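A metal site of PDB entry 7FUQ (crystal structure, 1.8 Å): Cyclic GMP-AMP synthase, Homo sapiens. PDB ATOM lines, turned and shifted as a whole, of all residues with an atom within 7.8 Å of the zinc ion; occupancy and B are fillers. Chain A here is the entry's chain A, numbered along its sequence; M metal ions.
The guanidinium group (NH2) of Arg 246 lies close to the side-chain sulfur (SG) of Cys 236 (3.8 Å).
The backbone carbonyl oxygen (O) of His 230 lies within hydrogen-bond range of the guanidinium group (NE) of Arg 246.
SG of Cys 244 sits close to NH2 of Arg 246 (3.5 Å).
N of Cys 237 sits at hydrogen-bond distance from O of Glu 242.
ND1 of His 230 is in hydrogen-bond range of O of Leu 227, at 2.9 Å.
Within 4 Å of the zinc ion: His 230, Cys 236, Cys 237 and Cys 244.
The nearest printed residue that does not touch the zinc ion is Arg 246 (4.4 Å).
A ring nitrogen (NE2) of His 230 binds the zinc ion, at 2.0 Å.
SG of Cys 237 binds the zinc ion, at 2.3 Å.
The zinc ion is bound by the side-chain sulfur (SG) of Cys 236, at 2.4 Å.
The side-chain sulfur (SG) of Cys 244 binds the zinc ion (2.4 Å).
The zinc ion has four donor atoms within binding distance.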
ATOM      1  N   LEU A 227      28.421   7.583  14.928  1.00  0.00           N
ATOM      2  CA  LEU A 227      27.330   6.665  15.227  1.00  0.00           C
ATOM      3  C   LEU A 227      26.345   7.261  16.222  1.00  0.00           C
ATOM      4  O   LEU A 227      25.135   7.015  16.108  1.00  0.00           O
ATOM      5  CB  LEU A 227      27.874   5.332  15.709  1.00  0.00           C
ATOM      6  CG  LEU A 227      26.859   4.203  15.864  1.00  0.00           C
ATOM      7  CD1 LEU A 227      26.139   3.923  14.548  1.00  0.00           C
ATOM      8  CD2 LEU A 227      27.591   2.960  16.379  1.00  0.00           C
ATOM      9  N   ASN A 229      25.950  10.552  16.590  1.00  0.00           N
ATOM     10  CA  ASN A 229      25.586  11.877  16.127  1.00  0.00           C
ATOM     11  C   ASN A 229      25.338  11.703  14.634  1.00  0.00           C
ATOM     12  O   ASN A 229      26.051  12.224  13.774  1.00  0.00           O
ATOM     13  CB  ASN A 229      26.662  12.908  16.452  1.00  0.00           C
ATOM     14  CG  ASN A 229      26.164  14.348  16.323  1.00  0.00           C
ATOM     15  OD1 ASN A 229      25.043  14.609  15.874  1.00  0.00           O
ATOM     16  ND2 ASN A 229      27.012  15.300  16.698  1.00  0.00           N
ATOM     17  N   HIS A 230      24.296  10.911  14.311  1.00  0.00           N
ATOM     18  CA  HIS A 230      24.211  10.216  13.040  1.00  0.00           C
ATOM     19  C   HIS A 230      23.196  10.796  12.072  1.00  0.00           C
ATOM     20  O   HIS A 230      23.015  10.230  10.981  1.00  0.00           O
ATOM     21  CB  HIS A 230      23.836   8.748  13.288  1.00  0.00           C
ATOM     22  CG  HIS A 230      22.542   8.581  14.043  1.00  0.00           C
ATOM     23  ND1 HIS A 230      22.482   7.986  15.273  1.00  0.00           N
ATOM     24  CD2 HIS A 230      21.283   8.974  13.748  1.00  0.00           C
ATOM     25  CE1 HIS A 230      21.231   8.004  15.716  1.00  0.00           C
ATOM     26  NE2 HIS A 230      20.483   8.611  14.812  1.00  0.00           N
ATOM     27  N   GLY A 231      22.449  11.823  12.456  1.00  0.00           N
ATOM     28  CA  GLY A 231      21.362  12.315  11.634  1.00  0.00           C
ATOM     29  C   GLY A 231      21.767  13.485  10.765  1.00  0.00           C
ATOM     30  O   GLY A 231      22.756  14.160  11.035  1.00  0.00           O
ATOM     31  N   LYS A 232      21.014  13.709   9.684  1.00  0.00           N
ATOM     32  CA  LYS A 232      21.102  15.029   9.061  1.00  0.00           C
ATOM     33  C   LYS A 232      20.638  16.091  10.041  1.00  0.00           C
ATOM     34  O   LYS A 232      21.277  17.139  10.182  1.00  0.00           O
ATOM     35  CB  LYS A 232      20.285  15.093   7.769  1.00  0.00           C
ATOM     36  CG  LYS A 232      20.213  16.539   7.250  1.00  0.00           C
ATOM     37  CD  LYS A 232      19.721  16.649   5.800  1.00  0.00           C
ATOM     38  CE  LYS A 232      20.580  15.802   4.837  1.00  0.00           C
ATOM     39  NZ  LYS A 232      22.003  16.284   4.715  1.00  0.00           N
ATOM     40  N   SER A 233      19.575  15.794  10.779  1.00  0.00           N
ATOM     41  CA  SER A 233      19.143  16.698  11.835  1.00  0.00           C
ATOM     42  C   SER A 233      20.075  16.560  13.039  1.00  0.00           C
ATOM     43  O   SER A 233      20.386  15.438  13.460  1.00  0.00           O
ATOM     44  CB  SER A 233      17.717  16.413  12.259  1.00  0.00           C
ATOM     45  OG  SER A 233      17.423  17.075  13.470  1.00  0.00           O
ATOM     46  N   THR A 235      19.201  17.074  15.985  1.00  0.00           N
ATOM     47  CA  THR A 235      18.439  16.450  17.061  1.00  0.00           C
ATOM     48  C   THR A 235      17.872  15.081  16.684  1.00  0.00           C
ATOM     49  O   THR A 235      16.952  14.597  17.366  1.00  0.00           O
ATOM     50  CB  THR A 235      17.316  17.371  17.558  1.00  0.00           C
ATOM     51  OG1 THR A 235      16.618  17.938  16.438  1.00  0.00           O
ATOM     52  CG2 THR A 235      17.916  18.512  18.403  1.00  0.00           C
ATOM     53  N   CYS A 236      18.414  14.437  15.652  1.00  0.00           N
ATOM     54  CA  CYS A 236      17.987  13.065  15.354  1.00  0.00           C
ATOM     55  C   CYS A 236      18.148  12.181  16.592  1.00  0.00           C
ATOM     56  O   CYS A 236      19.204  12.159  17.225  1.00  0.00           O
ATOM     57  CB  CYS A 236      18.803  12.481  14.197  1.00  0.00           C
ATOM     58  SG  CYS A 236      18.107  10.960  13.462  1.00  0.00           S
ATOM     59  N   CYS A 237      17.073  11.468  16.960  1.00  0.00           N
ATOM     60  CA  CYS A 237      17.041  10.546  18.097  1.00  0.00           C
ATOM     61  C   CYS A 237      17.244  11.243  19.447  1.00  0.00           C
ATOM     62  O   CYS A 237      17.487  10.594  20.466  1.00  0.00           O
ATOM     63  CB  CYS A 237      18.045   9.402  17.920  1.00  0.00           C
ATOM     64  SG  CYS A 237      17.562   8.236  16.618  1.00  0.00           S
ATOM     65  N   GLU A 238      17.072  12.567  19.518  1.00  0.00           N
ATOM     66  CA  GLU A 238      17.074  13.296  20.770  1.00  0.00           C
ATOM     67  C   GLU A 238      15.675  13.629  21.281  1.00  0.00           C
ATOM     68  O   GLU A 238      15.545  14.233  22.341  1.00  0.00           O
ATOM     69  CB  GLU A 238      17.878  14.605  20.655  1.00  0.00           C
ATOM     70  CG  GLU A 238      19.371  14.387  20.725  1.00  0.00           C
ATOM     71  CD  GLU A 238      20.169  15.648  21.079  1.00  0.00           C
ATOM     72  OE1 GLU A 238      19.578  16.741  21.238  1.00  0.00           O
ATOM     73  OE2 GLU A 238      21.399  15.533  21.172  1.00  0.00           O
ATOM     74  N   GLU A 242      11.753  12.530  16.338  1.00  0.00           N
ATOM     75  CA  GLU A 242      12.823  12.255  15.386  1.00  0.00           C
ATOM     76  C   GLU A 242      13.499  10.936  15.750  1.00  0.00           C
ATOM     77  O   GLU A 242      14.624  10.929  16.259  1.00  0.00           O
ATOM     78  CB  GLU A 242      13.840  13.392  15.343  1.00  0.00           C
ATOM     79  CG  GLU A 242      13.278  14.783  15.077  1.00  0.00           C
ATOM     80  CD  GLU A 242      14.382  15.825  15.009  1.00  0.00           C
ATOM     81  OE1 GLU A 242      15.252  15.687  14.128  1.00  0.00           O
ATOM     82  OE2 GLU A 242      14.402  16.764  15.855  1.00  0.00           O
ATOM     83  N   LYS A 243      12.823   9.826  15.484  1.00  0.00           N
ATOM     84  CA  LYS A 243      13.338   8.485  15.796  1.00  0.00           C
ATOM     85  C   LYS A 243      13.695   7.779  14.484  1.00  0.00           C
ATOM     86  O   LYS A 243      12.810   7.458  13.690  1.00  0.00           O
ATOM     87  CB  LYS A 243      12.314   7.690  16.592  1.00  0.00           C
ATOM     88  CG  LYS A 243      12.142   8.154  18.025  1.00  0.00           C
ATOM     89  CD  LYS A 243      13.376   7.814  18.861  1.00  0.00           C
ATOM     90  CE  LYS A 243      13.422   8.602  20.172  1.00  0.00           C
ATOM     91  NZ  LYS A 243      14.710   8.366  20.896  1.00  0.00           N
ATOM     92  N   CYS A 244      14.985   7.553  14.256  1.00  0.00           N
ATOM     93  CA  CYS A 244      15.401   6.840  13.056  1.00  0.00           C
ATOM     94  C   CYS A 244      15.874   5.434  13.420  1.00  0.00           C
ATOM     95  O   CYS A 244      16.073   5.099  14.594  1.00  0.00           O
ATOM     96  CB  CYS A 244      16.491   7.590  12.293  1.00  0.00           C
ATOM     97  SG  CYS A 244      18.175   7.388  12.969  1.00  0.00           S
ATOM     98  N   CYS A 245      16.081   4.608  12.402  1.00  0.00           N
ATOM     99  CA  CYS A 245      16.502   3.232  12.635  1.00  0.00           C
ATOM    100  C   CYS A 245      17.935   2.955  12.209  1.00  0.00           C
ATOM    101  O   CYS A 245      18.278   1.804  11.953  1.00  0.00           O
ATOM    102  CB  CYS A 245      15.545   2.242  11.955  1.00  0.00           C
ATOM    103  SG  CYS A 245      15.447   2.324  10.143  1.00  0.00           S
ATOM    104  N   ARG A 246      18.792   3.983  12.151  1.00  0.00           N
ATOM    105  CA  ARG A 246      20.170   3.759  11.689  1.00  0.00           C
ATOM    106  C   ARG A 246      20.923   2.782  12.603  1.00  0.00           C
ATOM    107  O   ARG A 246      21.474   1.772  12.138  1.00  0.00           O
ATOM    108  CB  ARG A 246      20.909   5.101  11.611  1.00  0.00           C
ATOM    109  CG  ARG A 246      20.520   5.959  10.390  1.00  0.00           C
ATOM    110  CD  ARG A 246      21.457   7.162  10.271  1.00  0.00           C
ATOM    111  NE  ARG A 246      21.157   8.100   9.201  1.00  0.00           N
ATOM    112  CZ  ARG A 246      20.295   9.115   9.312  1.00  0.00           C
ATOM    113  NH1 ARG A 246      20.138   9.972   8.308  1.00  0.00           N
ATOM    114  NH2 ARG A 246      19.591   9.272  10.429  1.00  0.00           N
ATOM    115  N   LYS A 247      20.939   3.046  13.914  1.00  0.00           N
ATOM    116  CA  LYS A 247      21.654   2.192  14.839  1.00  0.00           C
ATOM    117  C   LYS A 247      21.115   0.764  14.813  1.00  0.00           C
ATOM    118  O   LYS A 247      21.890  -0.198  14.855  1.00  0.00           O
ATOM    119  CB  LYS A 247      21.560   2.752  16.256  1.00  0.00           C
ATOM    120  CG  LYS A 247      22.512   3.908  16.514  1.00  0.00           C
ATOM    121  CD  LYS A 247      22.429   4.323  17.983  1.00  0.00           C
ATOM    122  CE  LYS A 247      23.517   5.303  18.362  1.00  0.00           C
ATOM    123  NZ  LYS A 247      23.354   5.877  19.757  1.00  0.00           N
ATOM    124  N   ASP A 292      17.137  11.915   6.948  1.00  0.00           N
ATOM    125  CA  ASP A 292      16.571  11.175   8.078  1.00  0.00           C
ATOM    126  C   ASP A 292      15.260  10.477   7.697  1.00  0.00           C
ATOM    127  O   ASP A 292      14.936   9.413   8.231  1.00  0.00           O
ATOM    128  CB  ASP A 292      16.363  12.120   9.265  1.00  0.00           C
ATOM    129  CG  ASP A 292      17.674  12.666   9.818  1.00  0.00           C
ATOM    130  OD1 ASP A 292      18.727  12.019   9.631  1.00  0.00           O
ATOM    131  OD2 ASP A 292      17.652  13.747  10.464  1.00  0.00           O
ATOM    132  N   TRP A 295      15.324   6.837   6.896  1.00  0.00           N
ATOM    133  CA  TRP A 295      15.614   5.932   8.004  1.00  0.00           C
ATOM    134  C   TRP A 295      14.501   5.976   9.045  1.00  0.00           C
ATOM    135  O   TRP A 295      14.738   5.781  10.228  1.00  0.00           O
ATOM    136  CB  TRP A 295      16.971   6.258   8.640  1.00  0.00           C
ATOM    137  CG  TRP A 295      18.128   6.128   7.689  1.00  0.00           C
ATOM    138  CD1 TRP A 295      18.644   7.102   6.857  1.00  0.00           C
ATOM    139  CD2 TRP A 295      18.896   4.953   7.454  1.00  0.00           C
ATOM    140  NE1 TRP A 295      19.688   6.578   6.124  1.00  0.00           N
ATOM    141  CE2 TRP A 295      19.862   5.267   6.470  1.00  0.00           C
ATOM    142  CE3 TRP A 295      18.848   3.650   7.964  1.00  0.00           C
ATOM    143  CZ2 TRP A 295      20.793   4.336   6.008  1.00  0.00           C
ATOM    144  CZ3 TRP A 295      19.789   2.707   7.506  1.00  0.00           C
ATOM    145  CH2 TRP A 295      20.728   3.046   6.528  1.00  0.00           C
HETATM  146 ZN    ZN M   1      18.562   8.985  14.656  1.00  0.00          ZN
